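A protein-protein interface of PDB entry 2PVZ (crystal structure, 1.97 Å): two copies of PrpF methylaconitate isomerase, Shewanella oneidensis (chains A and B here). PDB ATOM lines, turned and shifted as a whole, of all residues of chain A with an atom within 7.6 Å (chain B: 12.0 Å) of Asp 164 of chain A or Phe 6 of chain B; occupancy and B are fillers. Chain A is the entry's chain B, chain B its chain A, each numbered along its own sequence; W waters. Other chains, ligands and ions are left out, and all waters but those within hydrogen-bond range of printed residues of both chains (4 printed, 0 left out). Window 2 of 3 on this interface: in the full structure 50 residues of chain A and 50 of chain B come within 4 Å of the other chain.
Among the printed residues, pairs that only touch across the chains: Thr 162 of chain A with Gln 9 of chain B, Gly 163 of chain A with Phe 6 of chain B, Asp 164 of chain A with Phe 6 of chain B and Phe 172 of chain A with Arg 49 of chain B.
Gly 163 of chain A touches just one residue of chain B: Phe 6. Of chain B, only Phe 6 comes within 4 Å of Asp 164 of chain A. No residue of chain B comes within 4 Å of Phe 165 of chain A. No residue of chain B comes within 4 Å of Glu 166 of chain A. No residue of chain B comes within 4 Å of Ala 174 of chain A. Ala 175 of chain A touches none of the printed residues of chain B. Of the printed residues of chain A, Phe 6 of chain B touches Gln 160 (2.9 Å), Thr 162 (3.4 Å), Gly 163 (3.7 Å) and Asp 164 (3.6 Å). Of the printed residues of chain A, Gln 9 of chain B touches Glu 161 (2.8 Å) and Thr 162 (3.8 Å). Of the printed residues of chain A, Arg 49 of chain B touches Phe 172. Printed residues of chain A within 4 Å of Arg 393 of chain B: Glu 161. The nearest residue of chain A that does not touch Phe 6 of chain B is Thr 155 of chain A (5.9 Å).
No position is printed for both chains. Of the 10 pairs that touch across the chains among the printed residues, none has its exchanged pair printed and touching as well.
Of the 14 printed residues of chain A, 6 touch a printed residue of chain B. Hydrophobic or aromatic side chains of chain A that line the printed part of chain B: Phe 172. Of the 13 printed residues of chain B, 6 touch a printed residue of chain A. Among the printed residues, 10 pairs touch across the chains. Among the printed residues, Asp or Glu carboxylates within 4 Å of a Lys or Arg side-chain nitrogen of the other chain: Glu 161 of chain A with Arg 393 of chain B (3.0 Å).
The side-chain hydroxyl (OG1) of Thr 155 of chain A lies within hydrogen-bond range of the side-chain amide oxygen (OE1) of Gln 160 of chain A, at 2.6 Å. The side-chain amide nitrogen (NE2) of Gln 160 of chain A is in hydrogen-bond range of the backbone carbonyl oxygen (O) of Thr 162 of chain A (2.9 Å). N of Ala 175 of chain A is in hydrogen-bond range of O of Glu 161 of chain A (2.9 Å). NH2 of Arg 49 of chain B is in salt-bridge range of OD2 of Asp 62 of chain B, at 3.5 Å.
Water W2 bridges the side-chain carboxylate of Asp 62 of chain B (2.5 Å) and the backbone carbonyl oxygen of Phe 172 of chain A (3.0 Å). Water W4 bridges OE1 of Glu 161 of chain A (2.7 Å) and N of Gln 9 of chain B (2.9 Å). Water W3 lies within hydrogen-bond range of O of Pro 173 of chain A (2.8 Å) and NH2 of Arg 49 of chain B (2.9 Å). Water W1 lies within hydrogen-bond range of the backbone NH of Leu 5 of chain B, the side-chain amide oxygen of Gln 160 of chain A and the backbone NH of Phe 6 of chain B.
The side-chain carboxylate (OE1) of Glu 161 of chain A lies within salt-bridge range of the guanidinium group (NH1) of Arg 393 of chain B, 3.0 Å away. O of Phe 6 of chain B sits at hydrogen-bond distance from NE2 of Gln 160 of chain A, at 2.9 Å. The backbone carbonyl oxygen (O) of Pro 7 of chain B is in hydrogen-bond range of the side-chain hydroxyl (OG1) of Thr 162 of chain A (2.7 Å). The backbone NH (N) of Phe 172 of chain A sits close to the side-chain carboxylate (OD2) of Asp 62 of chain B (3.3 Å). The backbone carbonyl oxygen (O) of Phe 6 of chain B lies close to the side-chain hydroxyl (OG1) of Thr 162 of chain A (3.4 Å). The side-chain amide nitrogen of Gln 9 of chain B sits at hydrogen-bond distance from the side-chain carboxylate of Glu 161 of chain A.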
ATOM      1  N   THR A 155     -32.578  12.691 -20.397  1.00  0.00           N
ATOM      2  CA  THR A 155     -33.830  13.365 -20.750  1.00  0.00           C
ATOM      3  C   THR A 155     -34.495  12.606 -21.892  1.00  0.00           C
ATOM      4  O   THR A 155     -33.868  12.339 -22.928  1.00  0.00           O
ATOM      5  CB  THR A 155     -33.600  14.837 -21.154  1.00  0.00           C
ATOM      6  OG1 THR A 155     -32.981  15.539 -20.068  1.00  0.00           O
ATOM      7  CG2 THR A 155     -34.919  15.536 -21.503  1.00  0.00           C
ATOM      8  N   GLN A 160     -28.624  13.535 -21.820  1.00  0.00           N
ATOM      9  CA  GLN A 160     -28.694  14.983 -21.821  1.00  0.00           C
ATOM     10  C   GLN A 160     -27.263  15.513 -21.982  1.00  0.00           C
ATOM     11  O   GLN A 160     -26.476  15.486 -21.030  1.00  0.00           O
ATOM     12  CB  GLN A 160     -29.328  15.489 -20.513  1.00  0.00           C
ATOM     13  CG  GLN A 160     -29.395  17.011 -20.371  1.00  0.00           C
ATOM     14  CD  GLN A 160     -30.383  17.656 -21.327  1.00  0.00           C
ATOM     15  OE1 GLN A 160     -31.533  17.226 -21.432  1.00  0.00           O
ATOM     16  NE2 GLN A 160     -29.939  18.693 -22.033  1.00  0.00           N
ATOM     17  N   GLU A 161     -26.927  15.967 -23.189  1.00  0.00           N
ATOM     18  CA  GLU A 161     -25.578  16.471 -23.472  1.00  0.00           C
ATOM     19  C   GLU A 161     -25.412  17.937 -23.094  1.00  0.00           C
ATOM     20  O   GLU A 161     -24.366  18.344 -22.582  1.00  0.00           O
ATOM     21  CB  GLU A 161     -25.239  16.355 -24.959  1.00  0.00           C
ATOM     22  CG  GLU A 161     -25.258  14.967 -25.545  1.00  0.00           C
ATOM     23  CD  GLU A 161     -24.711  14.971 -26.958  1.00  0.00           C
ATOM     24  OE1 GLU A 161     -25.437  15.409 -27.883  1.00  0.00           O
ATOM     25  OE2 GLU A 161     -23.549  14.543 -27.128  1.00  0.00           O
ATOM     26  N   THR A 162     -26.440  18.724 -23.396  1.00  0.00           N
ATOM     27  CA  THR A 162     -26.380  20.175 -23.294  1.00  0.00           C
ATOM     28  C   THR A 162     -26.748  20.620 -21.882  1.00  0.00           C
ATOM     29  O   THR A 162     -27.451  19.909 -21.171  1.00  0.00           O
ATOM     30  CB  THR A 162     -27.334  20.834 -24.318  1.00  0.00           C
ATOM     31  OG1 THR A 162     -28.664  20.331 -24.120  1.00  0.00           O
ATOM     32  CG2 THR A 162     -26.900  20.501 -25.743  1.00  0.00           C
ATOM     33  N   GLY A 163     -26.265  21.791 -21.479  1.00  0.00           N
ATOM     34  CA  GLY A 163     -26.530  22.309 -20.140  1.00  0.00           C
ATOM     35  C   GLY A 163     -25.745  23.575 -19.872  1.00  0.00           C
ATOM     36  O   GLY A 163     -25.166  24.149 -20.795  1.00  0.00           O
ATOM     37  N   ASP A 164     -25.717  24.007 -18.611  1.00  0.00           N
ATOM     38  CA  ASP A 164     -25.058  25.266 -18.246  1.00  0.00           C
ATOM     39  C   ASP A 164     -23.832  25.100 -17.347  1.00  0.00           C
ATOM     40  O   ASP A 164     -23.352  26.071 -16.759  1.00  0.00           O
ATOM     41  CB  ASP A 164     -26.061  26.265 -17.632  1.00  0.00           C
ATOM     42  CG  ASP A 164     -26.716  25.755 -16.350  1.00  0.00           C
ATOM     43  OD1 ASP A 164     -26.364  24.662 -15.848  1.00  0.00           O
ATOM     44  OD2 ASP A 164     -27.613  26.463 -15.840  1.00  0.00           O
ATOM     45  N   PHE A 165     -23.320  23.874 -17.253  1.00  0.00           N
ATOM     46  CA  PHE A 165     -22.142  23.606 -16.429  1.00  0.00           C
ATOM     47  C   PHE A 165     -20.875  24.010 -17.174  1.00  0.00           C
ATOM     48  O   PHE A 165     -20.626  23.548 -18.288  1.00  0.00           O
ATOM     49  CB  PHE A 165     -22.090  22.128 -16.032  1.00  0.00           C
ATOM     50  CG  PHE A 165     -20.910  21.760 -15.170  1.00  0.00           C
ATOM     51  CD1 PHE A 165     -20.884  22.092 -13.822  1.00  0.00           C
ATOM     52  CD2 PHE A 165     -19.843  21.042 -15.703  1.00  0.00           C
ATOM     53  CE1 PHE A 165     -19.802  21.733 -13.021  1.00  0.00           C
ATOM     54  CE2 PHE A 165     -18.758  20.681 -14.910  1.00  0.00           C
ATOM     55  CZ  PHE A 165     -18.738  21.029 -13.569  1.00  0.00           C
ATOM     56  N   GLU A 166     -20.082  24.875 -16.547  1.00  0.00           N
ATOM     57  CA  GLU A 166     -18.850  25.362 -17.145  1.00  0.00           C
ATOM     58  C   GLU A 166     -17.636  24.782 -16.432  1.00  0.00           C
ATOM     59  O   GLU A 166     -17.632  24.628 -15.207  1.00  0.00           O
ATOM     60  CB  GLU A 166     -18.808  26.897 -17.131  1.00  0.00           C
ATOM     61  CG  GLU A 166     -20.002  27.534 -17.848  1.00  0.00           C
ATOM     62  CD  GLU A 166     -19.739  28.927 -18.369  1.00  0.00           C
ATOM     63  OE1 GLU A 166     -18.705  29.137 -19.045  1.00  0.00           O
ATOM     64  OE2 GLU A 166     -20.586  29.809 -18.117  1.00  0.00           O
ATOM     65  N   LEU A 167     -16.618  24.442 -17.219  1.00  0.00           N
ATOM     66  CA  LEU A 167     -15.365  23.921 -16.700  1.00  0.00           C
ATOM     67  C   LEU A 167     -14.229  24.656 -17.390  1.00  0.00           C
ATOM     68  O   LEU A 167     -14.244  24.819 -18.613  1.00  0.00           O
ATOM     69  CB  LEU A 167     -15.263  22.422 -16.972  1.00  0.00           C
ATOM     70  N   PHE A 172     -17.314  25.906 -24.150  1.00  0.00           N
ATOM     71  CA  PHE A 172     -18.757  26.122 -24.077  1.00  0.00           C
ATOM     72  C   PHE A 172     -19.370  25.288 -22.955  1.00  0.00           C
ATOM     73  O   PHE A 172     -18.857  24.217 -22.644  1.00  0.00           O
ATOM     74  CB  PHE A 172     -19.409  25.771 -25.420  1.00  0.00           C
ATOM     75  CG  PHE A 172     -18.870  26.563 -26.582  1.00  0.00           C
ATOM     76  CD1 PHE A 172     -19.273  27.879 -26.793  1.00  0.00           C
ATOM     77  CD2 PHE A 172     -17.962  25.992 -27.465  1.00  0.00           C
ATOM     78  CE1 PHE A 172     -18.767  28.616 -27.861  1.00  0.00           C
ATOM     79  CE2 PHE A 172     -17.455  26.723 -28.545  1.00  0.00           C
ATOM     80  CZ  PHE A 172     -17.857  28.029 -28.741  1.00  0.00           C
ATOM     81  N   PRO A 173     -20.468  25.775 -22.342  1.00  0.00           N
ATOM     82  CA  PRO A 173     -21.126  24.979 -21.301  1.00  0.00           C
ATOM     83  C   PRO A 173     -21.823  23.730 -21.842  1.00  0.00           C
ATOM     84  O   PRO A 173     -22.190  23.677 -23.019  1.00  0.00           O
ATOM     85  CB  PRO A 173     -22.142  25.954 -20.689  1.00  0.00           C
ATOM     86  CG  PRO A 173     -22.398  26.972 -21.747  1.00  0.00           C
ATOM     87  CD  PRO A 173     -21.126  27.082 -22.547  1.00  0.00           C
ATOM     88  N   ALA A 174     -21.970  22.730 -20.973  1.00  0.00           N
ATOM     89  CA  ALA A 174     -22.646  21.480 -21.294  1.00  0.00           C
ATOM     90  C   ALA A 174     -23.246  20.904 -20.006  1.00  0.00           C
ATOM     91  O   ALA A 174     -23.156  21.531 -18.949  1.00  0.00           O
ATOM     92  CB  ALA A 174     -21.661  20.484 -21.937  1.00  0.00           C
ATOM     93  N   ALA A 175     -23.852  19.724 -20.086  1.00  0.00           N
ATOM     94  CA  ALA A 175     -24.414  19.083 -18.893  1.00  0.00           C
ATOM     95  C   ALA A 175     -23.312  18.572 -17.972  1.00  0.00           C
ATOM     96  O   ALA A 175     -22.322  17.998 -18.433  1.00  0.00           O
ATOM     97  CB  ALA A 175     -25.353  17.946 -19.283  1.00  0.00           C
ATOM     98  N   GLU A 176     -23.484  18.788 -16.670  1.00  0.00           N
ATOM     99  CA  GLU A 176     -22.559  18.259 -15.673  1.00  0.00           C
ATOM    100  C   GLU A 176     -22.668  16.742 -15.589  1.00  0.00           C
ATOM    101  O   GLU A 176     -23.779  16.181 -15.546  1.00  0.00           O
ATOM    102  CB  GLU A 176     -22.820  18.878 -14.289  1.00  0.00           C
ATOM    103  CG  GLU A 176     -21.861  18.383 -13.193  1.00  0.00           C
ATOM    104  CD  GLU A 176     -22.033  19.114 -11.861  1.00  0.00           C
ATOM    105  OE1 GLU A 176     -22.942  19.966 -11.747  1.00  0.00           O
ATOM    106  OE2 GLU A 176     -21.241  18.842 -10.935  1.00  0.00           O
ATOM    107  N   LEU B   5     -35.112  21.716 -20.091  1.00  0.00           N
ATOM    108  CA  LEU B   5     -34.746  23.161 -20.170  1.00  0.00           C
ATOM    109  C   LEU B   5     -33.590  23.439 -21.151  1.00  0.00           C
ATOM    110  O   LEU B   5     -33.396  24.582 -21.573  1.00  0.00           O
ATOM    111  CB  LEU B   5     -34.464  23.740 -18.768  1.00  0.00           C
ATOM    112  CG  LEU B   5     -33.282  23.286 -17.900  1.00  0.00           C
ATOM    113  CD1 LEU B   5     -32.918  24.379 -16.890  1.00  0.00           C
ATOM    114  CD2 LEU B   5     -33.534  21.959 -17.192  1.00  0.00           C
ATOM    115  N   PHE B   6     -32.841  22.393 -21.508  1.00  0.00           N
ATOM    116  CA  PHE B   6     -31.801  22.474 -22.547  1.00  0.00           C
ATOM    117  C   PHE B   6     -32.091  21.449 -23.646  1.00  0.00           C
ATOM    118  O   PHE B   6     -31.986  20.243 -23.406  1.00  0.00           O
ATOM    119  CB  PHE B   6     -30.407  22.226 -21.947  1.00  0.00           C
ATOM    120  CG  PHE B   6     -29.957  23.301 -20.999  1.00  0.00           C
ATOM    121  CD1 PHE B   6     -29.283  24.424 -21.469  1.00  0.00           C
ATOM    122  CD2 PHE B   6     -30.204  23.190 -19.634  1.00  0.00           C
ATOM    123  CE1 PHE B   6     -28.867  25.428 -20.590  1.00  0.00           C
ATOM    124  CE2 PHE B   6     -29.791  24.190 -18.751  1.00  0.00           C
ATOM    125  CZ  PHE B   6     -29.124  25.308 -19.233  1.00  0.00           C
ATOM    126  N   PRO B   7     -32.460  21.921 -24.856  1.00  0.00           N
ATOM    127  CA  PRO B   7     -32.801  21.003 -25.939  1.00  0.00           C
ATOM    128  C   PRO B   7     -31.590  20.185 -26.415  1.00  0.00           C
ATOM    129  O   PRO B   7     -30.445  20.596 -26.185  1.00  0.00           O
ATOM    130  CB  PRO B   7     -33.288  21.942 -27.057  1.00  0.00           C
ATOM    131  CG  PRO B   7     -32.621  23.234 -26.781  1.00  0.00           C
ATOM    132  CD  PRO B   7     -32.577  23.329 -25.277  1.00  0.00           C
ATOM    133  N   PRO B   8     -31.839  19.028 -27.058  1.00  0.00           N
ATOM    134  CA  PRO B   8     -30.716  18.256 -27.589  1.00  0.00           C
ATOM    135  C   PRO B   8     -29.975  19.005 -28.695  1.00  0.00           C
ATOM    136  O   PRO B   8     -30.528  19.927 -29.304  1.00  0.00           O
ATOM    137  CB  PRO B   8     -31.379  16.996 -28.161  1.00  0.00           C
ATOM    138  CG  PRO B   8     -32.833  17.359 -28.349  1.00  0.00           C
ATOM    139  CD  PRO B   8     -33.141  18.378 -27.307  1.00  0.00           C
ATOM    140  N   GLN B   9     -28.727  18.606 -28.934  1.00  0.00           N
ATOM    141  CA  GLN B   9     -27.962  19.059 -30.086  1.00  0.00           C
ATOM    142  C   GLN B   9     -28.684  18.688 -31.369  1.00  0.00           C
ATOM    143  O   GLN B   9     -29.357  17.654 -31.441  1.00  0.00           O
ATOM    144  CB  GLN B   9     -26.596  18.385 -30.109  1.00  0.00           C
ATOM    145  CG  GLN B   9     -25.703  18.722 -28.926  1.00  0.00           C
ATOM    146  CD  GLN B   9     -24.251  18.518 -29.261  1.00  0.00           C
ATOM    147  OE1 GLN B   9     -23.548  19.468 -29.604  1.00  0.00           O
ATOM    148  NE2 GLN B   9     -23.792  17.268 -29.186  1.00  0.00           N
ATOM    149  N   ILE B  10     -28.535  19.531 -32.382  1.00  0.00           N
ATOM    150  CA  ILE B  10     -29.006  19.200 -33.716  1.00  0.00           C
ATOM    151  C   ILE B  10     -27.920  18.386 -34.439  1.00  0.00           C
ATOM    152  O   ILE B  10     -26.745  18.435 -34.061  1.00  0.00           O
ATOM    153  CB  ILE B  10     -29.387  20.474 -34.521  1.00  0.00           C
ATOM    154  CG1 ILE B  10     -28.183  21.407 -34.688  1.00  0.00           C
ATOM    155  CG2 ILE B  10     -30.559  21.200 -33.844  1.00  0.00           C
ATOM    156  CD1 ILE B  10     -28.270  22.366 -35.891  1.00  0.00           C
ATOM    157  N   ARG B  49     -19.585  27.296 -34.327  1.00  0.00           N
ATOM    158  CA  ARG B  49     -19.873  26.296 -33.306  1.00  0.00           C
ATOM    159  C   ARG B  49     -19.421  24.902 -33.732  1.00  0.00           C
ATOM    160  O   ARG B  49     -18.883  24.155 -32.922  1.00  0.00           O
ATOM    161  CB  ARG B  49     -21.357  26.308 -32.928  1.00  0.00           C
ATOM    162  CG  ARG B  49     -21.687  25.564 -31.640  1.00  0.00           C
ATOM    163  CD  ARG B  49     -21.024  26.196 -30.409  1.00  0.00           C
ATOM    164  NE  ARG B  49     -21.051  25.266 -29.284  1.00  0.00           N
ATOM    165  CZ  ARG B  49     -20.177  24.279 -29.104  1.00  0.00           C
ATOM    166  NH1 ARG B  49     -19.174  24.083 -29.970  1.00  0.00           N
ATOM    167  NH2 ARG B  49     -20.303  23.493 -28.048  1.00  0.00           N
ATOM    168  N   ASP B  62     -13.533  21.899 -28.140  1.00  0.00           N
ATOM    169  CA  ASP B  62     -14.991  21.760 -28.148  1.00  0.00           C
ATOM    170  C   ASP B  62     -15.585  21.960 -29.554  1.00  0.00           C
ATOM    171  O   ASP B  62     -16.624  22.609 -29.726  1.00  0.00           O
ATOM    172  CB  ASP B  62     -15.601  22.729 -27.129  1.00  0.00           C
ATOM    173  CG  ASP B  62     -16.939  22.260 -26.599  1.00  0.00           C
ATOM    174  OD1 ASP B  62     -17.343  21.115 -26.896  1.00  0.00           O
ATOM    175  OD2 ASP B  62     -17.577  23.041 -25.861  1.00  0.00           O
ATOM    176  N   ARG B 393     -22.579  17.559 -34.698  1.00  0.00           N
ATOM    177  CA  ARG B 393     -23.586  18.062 -33.766  1.00  0.00           C
ATOM    178  C   ARG B 393     -23.185  19.393 -33.163  1.00  0.00           C
ATOM    179  O   ARG B 393     -22.011  19.613 -32.848  1.00  0.00           O
ATOM    180  CB  ARG B 393     -23.804  17.073 -32.628  1.00  0.00           C
ATOM    181  CG  ARG B 393     -24.352  15.730 -33.039  1.00  0.00           C
ATOM    182  CD  ARG B 393     -24.877  15.018 -31.800  1.00  0.00           C
ATOM    183  NE  ARG B 393     -25.168  13.605 -32.039  1.00  0.00           N
ATOM    184  CZ  ARG B 393     -25.493  12.739 -31.080  1.00  0.00           C
ATOM    185  NH1 ARG B 393     -25.573  13.139 -29.820  1.00  0.00           N
ATOM    186  NH2 ARG B 393     -25.749  11.473 -31.381  1.00  0.00           N
ATOM    187  N   VAL B 394     -24.174  20.270 -32.999  1.00  0.00           N
ATOM    188  CA  VAL B 394     -24.028  21.502 -32.235  1.00  0.00           C
ATOM    189  C   VAL B 394     -25.294  21.699 -31.400  1.00  0.00           C
ATOM    190  O   VAL B 394     -26.344  21.159 -31.743  1.00  0.00           O
ATOM    191  CB  VAL B 394     -23.791  22.753 -33.134  1.00  0.00           C
ATOM    192  CG1 VAL B 394     -22.416  22.696 -33.817  1.00  0.00           C
ATOM    193  CG2 VAL B 394     -24.904  22.916 -34.160  1.00  0.00           C
ATOM    194  N   PRO B 395     -25.203  22.461 -30.298  1.00  0.00           N
ATOM    195  CA  PRO B 395     -26.428  22.794 -29.573  1.00  0.00           C
ATOM    196  C   PRO B 395     -27.445  23.484 -30.483  1.00  0.00           C
ATOM    197  O   PRO B 395     -27.061  24.160 -31.454  1.00  0.00           O
ATOM    198  CB  PRO B 395     -25.937  23.757 -28.483  1.00  0.00           C
ATOM    199  CG  PRO B 395     -24.512  23.356 -28.259  1.00  0.00           C
ATOM    200  CD  PRO B 395     -24.010  23.035 -29.642  1.00  0.00           C
ATOM    201  N   LYS B 396     -28.727  23.293 -30.182  1.00  0.00           N
ATOM    202  CA  LYS B 396     -29.795  23.928 -30.939  1.00  0.00           C
ATOM    203  C   LYS B 396     -29.542  25.439 -31.012  1.00  0.00           C
ATOM    204  O   LYS B 396     -29.398  26.087 -29.977  1.00  0.00           O
ATOM    205  CB  LYS B 396     -31.158  23.638 -30.303  1.00  0.00           C
ATOM    206  CG  LYS B 396     -32.342  23.994 -31.211  1.00  0.00           C
ATOM    207  CD  LYS B 396     -33.663  23.942 -30.456  1.00  0.00           C
ATOM    208  CE  LYS B 396     -34.770  24.669 -31.226  1.00  0.00           C
ATOM    209  NZ  LYS B 396     -35.995  24.864 -30.391  1.00  0.00           N
ATOM    210  N   PRO B 397     -29.441  25.990 -32.237  1.00  0.00           N
ATOM    211  CA  PRO B 397     -29.240  27.428 -32.457  1.00  0.00           C
ATOM    212  C   PRO B 397     -30.365  28.293 -31.881  1.00  0.00           C
ATOM    213  O   PRO B 397     -31.521  27.878 -31.771  1.00  0.00           O
ATOM    214  CB  PRO B 397     -29.219  27.546 -33.984  1.00  0.00           C
ATOM    215  CG  PRO B 397     -28.796  26.191 -34.455  1.00  0.00           C
ATOM    216  CD  PRO B 397     -29.476  25.248 -33.511  1.00  0.00           C
HETATM  217  O   HOH W   1     -33.264  19.512 -20.400  1.00  0.00           O
HETATM  218  O   HOH W   2     -19.461  22.030 -24.617  1.00  0.00           O
HETATM  219  O   HOH W   3     -21.829  22.874 -25.698  1.00  0.00           O
HETATM  220  O   HOH W   4     -27.988  16.121 -27.636  1.00  0.00           O
